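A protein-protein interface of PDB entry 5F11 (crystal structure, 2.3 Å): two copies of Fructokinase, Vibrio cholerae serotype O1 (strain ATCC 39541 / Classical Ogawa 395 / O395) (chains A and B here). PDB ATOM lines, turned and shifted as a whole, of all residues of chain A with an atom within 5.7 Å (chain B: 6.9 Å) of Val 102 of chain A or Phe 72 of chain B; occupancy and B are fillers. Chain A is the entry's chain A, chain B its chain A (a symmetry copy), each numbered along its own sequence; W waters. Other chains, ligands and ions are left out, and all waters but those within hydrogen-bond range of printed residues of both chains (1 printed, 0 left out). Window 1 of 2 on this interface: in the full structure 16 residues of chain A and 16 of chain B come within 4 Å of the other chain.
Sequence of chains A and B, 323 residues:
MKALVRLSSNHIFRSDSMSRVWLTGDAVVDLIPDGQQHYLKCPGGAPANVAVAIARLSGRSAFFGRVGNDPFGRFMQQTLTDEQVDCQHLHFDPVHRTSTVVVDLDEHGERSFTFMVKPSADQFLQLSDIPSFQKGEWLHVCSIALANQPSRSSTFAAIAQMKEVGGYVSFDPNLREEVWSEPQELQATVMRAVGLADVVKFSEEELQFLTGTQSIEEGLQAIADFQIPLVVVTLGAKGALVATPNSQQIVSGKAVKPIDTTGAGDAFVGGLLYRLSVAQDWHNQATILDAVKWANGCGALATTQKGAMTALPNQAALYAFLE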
ATOM      1  N   VAL A  29      -5.694  12.370 -21.124  1.00  0.00           N
ATOM      2  CA  VAL A  29      -6.289  12.352 -19.804  1.00  0.00           C
ATOM      3  C   VAL A  29      -7.034  11.037 -19.623  1.00  0.00           C
ATOM      4  O   VAL A  29      -7.977  10.735 -20.369  1.00  0.00           O
ATOM      5  CB  VAL A  29      -7.247  13.532 -19.601  1.00  0.00           C
ATOM      6  CG1 VAL A  29      -7.887  13.454 -18.227  1.00  0.00           C
ATOM      7  CG2 VAL A  29      -6.501  14.835 -19.763  1.00  0.00           C
ATOM      8  N   LEU A  31      -9.478   8.816 -17.588  1.00  0.00           N
ATOM      9  CA  LEU A  31     -10.579   8.786 -16.644  1.00  0.00           C
ATOM     10  C   LEU A  31     -10.612   7.384 -16.054  1.00  0.00           C
ATOM     11  O   LEU A  31     -10.811   6.404 -16.771  1.00  0.00           O
ATOM     12  CB  LEU A  31     -11.901   9.111 -17.348  1.00  0.00           C
ATOM     13  CG  LEU A  31     -12.348  10.573 -17.491  1.00  0.00           C
ATOM     14  CD1 LEU A  31     -11.259  11.569 -17.140  1.00  0.00           C
ATOM     15  CD2 LEU A  31     -12.865  10.845 -18.887  1.00  0.00           C
ATOM     16  N   TYR A  39     -14.665   9.582 -11.282  1.00  0.00           N
ATOM     17  CA  TYR A  39     -13.485   9.279 -12.071  1.00  0.00           C
ATOM     18  C   TYR A  39     -12.300  10.080 -11.510  1.00  0.00           C
ATOM     19  O   TYR A  39     -12.413  11.292 -11.305  1.00  0.00           O
ATOM     20  CB  TYR A  39     -13.714   9.652 -13.542  1.00  0.00           C
ATOM     21  CG  TYR A  39     -14.539   8.680 -14.364  1.00  0.00           C
ATOM     22  CD1 TYR A  39     -14.038   7.434 -14.725  1.00  0.00           C
ATOM     23  CD2 TYR A  39     -15.793   9.036 -14.835  1.00  0.00           C
ATOM     24  CE1 TYR A  39     -14.779   6.564 -15.495  1.00  0.00           C
ATOM     25  CE2 TYR A  39     -16.539   8.173 -15.596  1.00  0.00           C
ATOM     26  CZ  TYR A  39     -16.031   6.939 -15.925  1.00  0.00           C
ATOM     27  OH  TYR A  39     -16.786   6.083 -16.690  1.00  0.00           O
ATOM     28  N   THR A 100      -8.942  11.664 -24.768  1.00  0.00           N
ATOM     29  CA  THR A 100      -9.644  11.399 -23.518  1.00  0.00           C
ATOM     30  C   THR A 100     -10.070   9.931 -23.458  1.00  0.00           C
ATOM     31  O   THR A 100     -10.872   9.477 -24.278  1.00  0.00           O
ATOM     32  CB  THR A 100     -10.904  12.266 -23.407  1.00  0.00           C
ATOM     33  OG1 THR A 100     -10.545  13.651 -23.455  1.00  0.00           O
ATOM     34  CG2 THR A 100     -11.664  11.961 -22.106  1.00  0.00           C
ATOM     35  N   VAL A 101      -9.541   9.193 -22.489  1.00  0.00           N
ATOM     36  CA  VAL A 101      -9.769   7.754 -22.428  1.00  0.00           C
ATOM     37  C   VAL A 101     -10.411   7.311 -21.107  1.00  0.00           C
ATOM     38  O   VAL A 101     -10.001   7.724 -20.019  1.00  0.00           O
ATOM     39  CB  VAL A 101      -8.458   6.955 -22.672  1.00  0.00           C
ATOM     40  CG1 VAL A 101      -8.739   5.457 -22.770  1.00  0.00           C
ATOM     41  CG2 VAL A 101      -7.759   7.429 -23.937  1.00  0.00           C
ATOM     42  N   VAL A 102     -11.425   6.464 -21.227  1.00  0.00           N
ATOM     43  CA  VAL A 102     -12.097   5.865 -20.083  1.00  0.00           C
ATOM     44  C   VAL A 102     -11.497   4.490 -19.803  1.00  0.00           C
ATOM     45  O   VAL A 102     -11.459   3.634 -20.689  1.00  0.00           O
ATOM     46  CB  VAL A 102     -13.612   5.690 -20.361  1.00  0.00           C
ATOM     47  CG1 VAL A 102     -14.338   5.312 -19.090  1.00  0.00           C
ATOM     48  CG2 VAL A 102     -14.206   6.963 -20.941  1.00  0.00           C
ATOM     49  N   VAL A 103     -11.042   4.267 -18.574  1.00  0.00           N
ATOM     50  CA  VAL A 103     -10.478   2.969 -18.204  1.00  0.00           C
ATOM     51  C   VAL A 103     -11.489   2.015 -17.537  1.00  0.00           C
ATOM     52  O   VAL A 103     -12.247   2.406 -16.658  1.00  0.00           O
ATOM     53  CB  VAL A 103      -9.230   3.129 -17.305  1.00  0.00           C
ATOM     54  CG1 VAL A 103      -8.569   1.779 -17.059  1.00  0.00           C
ATOM     55  CG2 VAL A 103      -8.239   4.073 -17.936  1.00  0.00           C
ATOM     56  N   ASP A 104     -11.488   0.762 -17.981  1.00  0.00           N
ATOM     57  CA  ASP A 104     -12.233  -0.313 -17.326  1.00  0.00           C
ATOM     58  C   ASP A 104     -11.251  -1.232 -16.589  1.00  0.00           C
ATOM     59  O   ASP A 104     -10.523  -2.007 -17.210  1.00  0.00           O
ATOM     60  CB  ASP A 104     -13.018  -1.116 -18.364  1.00  0.00           C
ATOM     61  CG  ASP A 104     -13.887  -2.194 -17.742  1.00  0.00           C
ATOM     62  OD1 ASP A 104     -14.933  -2.515 -18.345  1.00  0.00           O
ATOM     63  OD2 ASP A 104     -13.546  -2.724 -16.664  1.00  0.00           O
ATOM     64  N   SER A 112      -8.707  -2.554 -22.023  1.00  0.00           N
ATOM     65  CA  SER A 112      -9.216  -1.784 -20.891  1.00  0.00           C
ATOM     66  C   SER A 112      -9.526  -0.341 -21.277  1.00  0.00           C
ATOM     67  O   SER A 112     -10.073   0.418 -20.479  1.00  0.00           O
ATOM     68  CB  SER A 112      -8.225  -1.819 -19.721  1.00  0.00           C
ATOM     69  OG  SER A 112      -7.006  -1.177 -20.071  1.00  0.00           O
ATOM     70  N   PHE A 113      -9.191   0.033 -22.505  1.00  0.00           N
ATOM     71  CA  PHE A 113      -9.367   1.416 -22.923  1.00  0.00           C
ATOM     72  C   PHE A 113     -10.548   1.685 -23.864  1.00  0.00           C
ATOM     73  O   PHE A 113     -10.851   0.902 -24.765  1.00  0.00           O
ATOM     74  CB  PHE A 113      -8.068   1.946 -23.521  1.00  0.00           C
ATOM     75  CG  PHE A 113      -6.899   1.812 -22.604  1.00  0.00           C
ATOM     76  CD1 PHE A 113      -5.924   0.857 -22.835  1.00  0.00           C
ATOM     77  CD2 PHE A 113      -6.784   2.621 -21.492  1.00  0.00           C
ATOM     78  CE1 PHE A 113      -4.842   0.725 -21.975  1.00  0.00           C
ATOM     79  CE2 PHE A 113      -5.703   2.493 -20.635  1.00  0.00           C
ATOM     80  CZ  PHE A 113      -4.733   1.539 -20.877  1.00  0.00           C
ATOM     81  N   THR A 114     -11.212   2.806 -23.632  1.00  0.00           N
ATOM     82  CA  THR A 114     -12.231   3.296 -24.536  1.00  0.00           C
ATOM     83  C   THR A 114     -11.836   4.706 -24.933  1.00  0.00           C
ATOM     84  O   THR A 114     -11.797   5.600 -24.092  1.00  0.00           O
ATOM     85  CB  THR A 114     -13.622   3.316 -23.876  1.00  0.00           C
ATOM     86  OG1 THR A 114     -13.943   2.003 -23.400  1.00  0.00           O
ATOM     87  CG2 THR A 114     -14.684   3.755 -24.874  1.00  0.00           C
ATOM     88  N   PHE A 115     -11.539   4.897 -26.215  1.00  0.00           N
ATOM     89  CA  PHE A 115     -11.059   6.184 -26.712  1.00  0.00           C
ATOM     90  C   PHE A 115     -12.222   7.087 -27.111  1.00  0.00           C
ATOM     91  O   PHE A 115     -12.967   6.759 -28.028  1.00  0.00           O
ATOM     92  CB  PHE A 115     -10.104   5.973 -27.893  1.00  0.00           C
ATOM     93  CG  PHE A 115      -8.773   5.390 -27.495  1.00  0.00           C
ATOM     94  CD1 PHE A 115      -7.647   6.189 -27.434  1.00  0.00           C
ATOM     95  CD2 PHE A 115      -8.659   4.047 -27.161  1.00  0.00           C
ATOM     96  CE1 PHE A 115      -6.437   5.666 -27.053  1.00  0.00           C
ATOM     97  CE2 PHE A 115      -7.463   3.517 -26.780  1.00  0.00           C
ATOM     98  CZ  PHE A 115      -6.341   4.327 -26.726  1.00  0.00           C
ATOM     99  N   MET A 116     -12.367   8.220 -26.422  1.00  0.00           N
ATOM    100  CA  MET A 116     -13.533   9.087 -26.596  1.00  0.00           C
ATOM    101  C   MET A 116     -13.369  10.165 -27.672  1.00  0.00           C
ATOM    102  O   MET A 116     -14.360  10.750 -28.129  1.00  0.00           O
ATOM    103  CB  MET A 116     -13.943   9.718 -25.266  1.00  0.00           C
ATOM    104  CG  MET A 116     -14.467   8.711 -24.249  1.00  0.00           C
ATOM    105  SD  MET A 116     -15.764   7.622 -24.899  1.00  0.00           S
ATOM    106  CE  MET A 116     -17.072   8.789 -25.292  1.00  0.00           C
ATOM    107  N   ALA B  27     -27.892  13.264 -25.970  1.00  0.00           N
ATOM    108  CA  ALA B  27     -27.774  12.706 -24.617  1.00  0.00           C
ATOM    109  C   ALA B  27     -26.291  12.709 -24.301  1.00  0.00           C
ATOM    110  O   ALA B  27     -25.499  12.227 -25.109  1.00  0.00           O
ATOM    111  CB  ALA B  27     -28.308  11.287 -24.565  1.00  0.00           C
ATOM    112  N   VAL B  28     -25.894  13.284 -23.166  1.00  0.00           N
ATOM    113  CA  VAL B  28     -24.466  13.385 -22.876  1.00  0.00           C
ATOM    114  C   VAL B  28     -24.090  13.042 -21.442  1.00  0.00           C
ATOM    115  O   VAL B  28     -24.874  13.210 -20.512  1.00  0.00           O
ATOM    116  CB  VAL B  28     -23.852  14.769 -23.271  1.00  0.00           C
ATOM    117  CG1 VAL B  28     -24.766  15.544 -24.231  1.00  0.00           C
ATOM    118  CG2 VAL B  28     -23.528  15.603 -22.045  1.00  0.00           C
ATOM    119  N   VAL B  29     -22.873  12.540 -21.285  1.00  0.00           N
ATOM    120  CA  VAL B  29     -22.305  12.309 -19.973  1.00  0.00           C
ATOM    121  C   VAL B  29     -21.566  13.565 -19.534  1.00  0.00           C
ATOM    122  O   VAL B  29     -20.609  14.000 -20.191  1.00  0.00           O
ATOM    123  CB  VAL B  29     -21.349  11.110 -19.975  1.00  0.00           C
ATOM    124  CG1 VAL B  29     -20.737  10.928 -18.598  1.00  0.00           C
ATOM    125  CG2 VAL B  29     -22.089   9.862 -20.393  1.00  0.00           C
ATOM    126  N   LEU B  31     -19.169  15.361 -17.069  1.00  0.00           N
ATOM    127  CA  LEU B  31     -18.088  15.211 -16.114  1.00  0.00           C
ATOM    128  C   LEU B  31     -18.069  16.478 -15.270  1.00  0.00           C
ATOM    129  O   LEU B  31     -17.857  17.574 -15.787  1.00  0.00           O
ATOM    130  CB  LEU B  31     -16.751  15.021 -16.839  1.00  0.00           C
ATOM    131  CG  LEU B  31     -16.298  13.611 -17.244  1.00  0.00           C
ATOM    132  CD1 LEU B  31     -17.392  12.570 -17.109  1.00  0.00           C
ATOM    133  CD2 LEU B  31     -15.752  13.605 -18.655  1.00  0.00           C
ATOM    134  N   LYS B  41     -19.701  11.264 -12.513  1.00  0.00           N
ATOM    135  CA  LYS B  41     -20.181  10.885 -13.832  1.00  0.00           C
ATOM    136  C   LYS B  41     -21.700  11.025 -13.821  1.00  0.00           C
ATOM    137  O   LYS B  41     -22.407  10.180 -13.264  1.00  0.00           O
ATOM    138  CB  LYS B  41     -19.760   9.458 -14.167  1.00  0.00           C
ATOM    139  CG  LYS B  41     -20.325   8.922 -15.472  1.00  0.00           C
ATOM    140  CD  LYS B  41     -20.806   7.491 -15.272  1.00  0.00           C
ATOM    141  CE  LYS B  41     -20.451   6.594 -16.441  1.00  0.00           C
ATOM    142  NZ  LYS B  41     -20.374   5.175 -15.995  1.00  0.00           N
ATOM    143  N   VAL B  67     -27.130   7.854 -29.924  1.00  0.00           N
ATOM    144  CA  VAL B  67     -25.977   7.894 -29.036  1.00  0.00           C
ATOM    145  C   VAL B  67     -24.915   7.001 -29.647  1.00  0.00           C
ATOM    146  O   VAL B  67     -25.157   6.387 -30.693  1.00  0.00           O
ATOM    147  CB  VAL B  67     -26.313   7.396 -27.591  1.00  0.00           C
ATOM    148  CG1 VAL B  67     -27.197   8.396 -26.862  1.00  0.00           C
ATOM    149  CG2 VAL B  67     -26.963   6.000 -27.616  1.00  0.00           C
ATOM    150  N   GLY B  68     -23.750   6.923 -29.010  1.00  0.00           N
ATOM    151  CA  GLY B  68     -22.678   6.088 -29.515  1.00  0.00           C
ATOM    152  C   GLY B  68     -22.825   4.649 -29.067  1.00  0.00           C
ATOM    153  O   GLY B  68     -23.401   4.376 -28.011  1.00  0.00           O
ATOM    154  N   ASN B  69     -22.302   3.715 -29.855  1.00  0.00           N
ATOM    155  CA  ASN B  69     -22.263   2.322 -29.419  1.00  0.00           C
ATOM    156  C   ASN B  69     -21.111   2.065 -28.443  1.00  0.00           C
ATOM    157  O   ASN B  69     -20.227   1.247 -28.707  1.00  0.00           O
ATOM    158  CB  ASN B  69     -22.152   1.381 -30.609  1.00  0.00           C
ATOM    159  CG  ASN B  69     -22.434  -0.048 -30.236  1.00  0.00           C
ATOM    160  OD1 ASN B  69     -23.154  -0.310 -29.276  1.00  0.00           O
ATOM    161  ND2 ASN B  69     -21.866  -0.986 -30.990  1.00  0.00           N
ATOM    162  N   ASP B  70     -21.133   2.764 -27.310  1.00  0.00           N
ATOM    163  CA  ASP B  70     -20.062   2.686 -26.322  1.00  0.00           C
ATOM    164  C   ASP B  70     -20.680   2.661 -24.923  1.00  0.00           C
ATOM    165  O   ASP B  70     -21.892   2.844 -24.798  1.00  0.00           O
ATOM    166  CB  ASP B  70     -19.136   3.888 -26.510  1.00  0.00           C
ATOM    167  CG  ASP B  70     -19.892   5.178 -26.705  1.00  0.00           C
ATOM    168  OD1 ASP B  70     -19.549   5.909 -27.653  1.00  0.00           O
ATOM    169  OD2 ASP B  70     -20.815   5.468 -25.910  1.00  0.00           O
ATOM    170  N   PRO B  71     -19.868   2.437 -23.870  1.00  0.00           N
ATOM    171  CA  PRO B  71     -20.438   2.382 -22.512  1.00  0.00           C
ATOM    172  C   PRO B  71     -21.249   3.620 -22.103  1.00  0.00           C
ATOM    173  O   PRO B  71     -22.300   3.465 -21.480  1.00  0.00           O
ATOM    174  CB  PRO B  71     -19.202   2.253 -21.620  1.00  0.00           C
ATOM    175  CG  PRO B  71     -18.214   1.565 -22.461  1.00  0.00           C
ATOM    176  CD  PRO B  71     -18.452   2.026 -23.878  1.00  0.00           C
ATOM    177  N   PHE B  72     -20.776   4.819 -22.439  1.00  0.00           N
ATOM    178  CA  PHE B  72     -21.520   6.045 -22.139  1.00  0.00           C
ATOM    179  C   PHE B  72     -22.917   6.020 -22.763  1.00  0.00           C
ATOM    180  O   PHE B  72     -23.902   6.402 -22.127  1.00  0.00           O
ATOM    181  CB  PHE B  72     -20.763   7.288 -22.626  1.00  0.00           C
ATOM    182  CG  PHE B  72     -19.646   7.715 -21.718  1.00  0.00           C
ATOM    183  CD1 PHE B  72     -19.321   6.970 -20.588  1.00  0.00           C
ATOM    184  CD2 PHE B  72     -18.929   8.869 -21.985  1.00  0.00           C
ATOM    185  CE1 PHE B  72     -18.288   7.364 -19.753  1.00  0.00           C
ATOM    186  CE2 PHE B  72     -17.908   9.277 -21.157  1.00  0.00           C
ATOM    187  CZ  PHE B  72     -17.584   8.526 -20.033  1.00  0.00           C
ATOM    188  N   GLY B  73     -22.990   5.569 -24.010  1.00  0.00           N
ATOM    189  CA  GLY B  73     -24.254   5.467 -24.712  1.00  0.00           C
ATOM    190  C   GLY B  73     -25.206   4.508 -24.029  1.00  0.00           C
ATOM    191  O   GLY B  73     -26.402   4.756 -23.938  1.00  0.00           O
ATOM    192  N   ARG B  74     -24.663   3.406 -23.536  1.00  0.00           N
ATOM    193  CA  ARG B  74     -25.467   2.394 -22.881  1.00  0.00           C
ATOM    194  C   ARG B  74     -25.907   2.882 -21.497  1.00  0.00           C
ATOM    195  O   ARG B  74     -27.028   2.623 -21.066  1.00  0.00           O
ATOM    196  CB  ARG B  74     -24.687   1.075 -22.799  1.00  0.00           C
ATOM    197  CG  ARG B  74     -24.638   0.307 -24.116  1.00  0.00           C
ATOM    198  CD  ARG B  74     -23.871  -1.002 -23.947  1.00  0.00           C
ATOM    199  NE  ARG B  74     -22.427  -0.824 -24.066  1.00  0.00           N
ATOM    200  CZ  ARG B  74     -21.738  -1.089 -25.171  1.00  0.00           C
ATOM    201  NH1 ARG B  74     -22.365  -1.557 -26.249  1.00  0.00           N
ATOM    202  NH2 ARG B  74     -20.428  -0.885 -25.198  1.00  0.00           N
ATOM    203  N   PHE B  75     -25.011   3.598 -20.825  1.00  0.00           N
ATOM    204  CA  PHE B  75     -25.305   4.269 -19.560  1.00  0.00           C
ATOM    205  C   PHE B  75     -26.441   5.288 -19.731  1.00  0.00           C
ATOM    206  O   PHE B  75     -27.325   5.397 -18.876  1.00  0.00           O
ATOM    207  CB  PHE B  75     -24.028   4.933 -19.032  1.00  0.00           C
ATOM    208  CG  PHE B  75     -24.233   5.821 -17.849  1.00  0.00           C
ATOM    209  CD1 PHE B  75     -24.304   5.292 -16.563  1.00  0.00           C
ATOM    210  CD2 PHE B  75     -24.311   7.198 -18.006  1.00  0.00           C
ATOM    211  CE1 PHE B  75     -24.477   6.114 -15.456  1.00  0.00           C
ATOM    212  CE2 PHE B  75     -24.489   8.037 -16.892  1.00  0.00           C
ATOM    213  CZ  PHE B  75     -24.567   7.492 -15.624  1.00  0.00           C
ATOM    214  N   MET B  76     -26.429   6.014 -20.844  1.00  0.00           N
ATOM    215  CA  MET B  76     -27.503   6.958 -21.145  1.00  0.00           C
ATOM    216  C   MET B  76     -28.816   6.252 -21.467  1.00  0.00           C
ATOM    217  O   MET B  76     -29.874   6.663 -20.993  1.00  0.00           O
ATOM    218  CB  MET B  76     -27.109   7.930 -22.254  1.00  0.00           C
ATOM    219  CG  MET B  76     -26.156   9.010 -21.786  1.00  0.00           C
ATOM    220  SD  MET B  76     -26.568   9.622 -20.119  1.00  0.00           S
ATOM    221  CE  MET B  76     -28.090  10.539 -20.374  1.00  0.00           C
ATOM    222  N   GLN B  77     -28.750   5.188 -22.263  1.00  0.00           N
ATOM    223  CA  GLN B  77     -29.927   4.361 -22.538  1.00  0.00           C
ATOM    224  C   GLN B  77     -30.568   3.853 -21.246  1.00  0.00           C
ATOM    225  O   GLN B  77     -31.747   4.073 -20.992  1.00  0.00           O
ATOM    226  CB  GLN B  77     -29.542   3.152 -23.389  1.00  0.00           C
ATOM    227  CG  GLN B  77     -30.660   2.123 -23.505  1.00  0.00           C
ATOM    228  CD  GLN B  77     -30.218   0.856 -24.204  1.00  0.00           C
ATOM    229  OE1 GLN B  77     -29.177   0.286 -23.869  1.00  0.00           O
ATOM    230  NE2 GLN B  77     -31.003   0.408 -25.185  1.00  0.00           N
ATOM    231  N   THR B  98     -20.326   8.850 -28.091  1.00  0.00           N
ATOM    232  CA  THR B  98     -21.340   9.532 -27.289  1.00  0.00           C
ATOM    233  C   THR B  98     -20.768  10.864 -26.817  1.00  0.00           C
ATOM    234  O   THR B  98     -19.579  10.945 -26.506  1.00  0.00           O
ATOM    235  CB  THR B  98     -21.765   8.684 -26.057  1.00  0.00           C
ATOM    236  OG1 THR B  98     -22.224   7.395 -26.491  1.00  0.00           O
ATOM    237  CG2 THR B  98     -22.887   9.363 -25.273  1.00  0.00           C
ATOM    238  N   SER B  99     -21.606  11.902 -26.784  1.00  0.00           N
ATOM    239  CA  SER B  99     -21.184  13.230 -26.337  1.00  0.00           C
ATOM    240  C   SER B  99     -20.644  13.188 -24.896  1.00  0.00           C
ATOM    241  O   SER B  99     -21.189  12.496 -24.028  1.00  0.00           O
ATOM    242  CB  SER B  99     -22.344  14.226 -26.471  1.00  0.00           C
ATOM    243  OG  SER B  99     -21.954  15.566 -26.206  1.00  0.00           O
ATOM    244  N   THR B 100     -19.552  13.910 -24.664  1.00  0.00           N
ATOM    245  CA  THR B 100     -18.877  13.935 -23.373  1.00  0.00           C
ATOM    246  C   THR B 100     -18.455  15.364 -23.031  1.00  0.00           C
ATOM    247  O   THR B 100     -17.637  15.963 -23.734  1.00  0.00           O
ATOM    248  CB  THR B 100     -17.618  13.060 -23.401  1.00  0.00           C
ATOM    249  OG1 THR B 100     -17.974  11.709 -23.715  1.00  0.00           O
ATOM    250  CG2 THR B 100     -16.886  13.114 -22.050  1.00  0.00           C
ATOM    251  N   VAL B 101     -19.005  15.909 -21.951  1.00  0.00           N
ATOM    252  CA  VAL B 101     -18.782  17.311 -21.617  1.00  0.00           C
ATOM    253  C   VAL B 101     -18.168  17.497 -20.224  1.00  0.00           C
ATOM    254  O   VAL B 101     -18.599  16.888 -19.241  1.00  0.00           O
ATOM    255  CB  VAL B 101     -20.089  18.144 -21.733  1.00  0.00           C
ATOM    256  CG1 VAL B 101     -19.809  19.633 -21.543  1.00  0.00           C
ATOM    257  CG2 VAL B 101     -20.761  17.917 -23.080  1.00  0.00           C
HETATM  258  O   HOH W   1     -18.054   5.275 -23.330  1.00  0.00           O
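N of Met 116 of chain A is in hydrogen-bond range of O of Thr 100 of chain A (2.9 Å). OD2 of Asp 70 of chain B is in hydrogen-bond range of OG1 of Thr 98 of chain B. N of Gly 73 of chain B is in hydrogen-bond range of OG1 of Thr 98 of chain B (3.2 Å). The side-chain hydroxyl (OG1) of Thr 98 of chain B lies within hydrogen-bond range of the backbone NH (N) of Gly 68 of chain B, 3.0 Å away. O of Thr 98 of chain B sits at hydrogen-bond distance from OG1 of Thr 100 of chain B, at 3.3 Å. The backbone NH (N) of Val 102 of chain A is in hydrogen-bond range of the backbone carbonyl oxygen (O) of Thr 114 of chain A.
Among the printed residues, pairs that only touch across the chains: Met 116 of chain A with Thr 100 of chain B, Met 116 of chain A with Thr 98 of chain B, Tyr 39 of chain A with Phe 72 of chain B, Tyr 39 of chain A with Lys 41 of chain B, Met 116 of chain A with Phe 72 of chain B and Val 102 of chain A with Phe 72 of chain B.
Printed residues of chain B within 4 Å of Tyr 39 of chain A: Lys 41 and Phe 72. Val 102 of chain A touches one residue of chain B. Val 103 of chain A touches none of the printed residues of chain B. Of the printed residues of chain B, Met 116 of chain A touches Phe 72 (3.8 Å), Thr 98 (3.5 Å) and Thr 100 (3.4 Å). Of chain A, only Tyr 39, Val 102 and Met 116 come within 4 Å of Phe 72 of chain B. Of the printed residues of chain A, Thr 100 of chain B touches Met 116. The nearest residue of chain A that does not touch Phe 72 of chain B is Leu 31 of chain A (5.4 Å).
Of the 20 printed residues of chain B, 4 touch a printed residue of chain A. Of the 13 printed residues of chain A, 3 touch a printed residue of chain B. Printed residues of chain A that touch a printed residue of chain B: Tyr 39, Val 102 and Met 116. Hydrophobic or aromatic side chains of chain A within 4 Å of the printed part of chain B: Tyr 39, Val 102 and Met 116. Along chain A the printed residues that touch a printed residue of chain B span positions 39 to 116. Among the printed residues, no Asp or Glu carboxylate lies within 4 Å of a Lys or Arg side-chain nitrogen of the other chain.
4 positions are printed for both chains.
Water W1 lies within hydrogen-bond range of N of Phe 72 of chain B (2.9 Å) and SD of Met 116 of chain A (3.6 Å).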
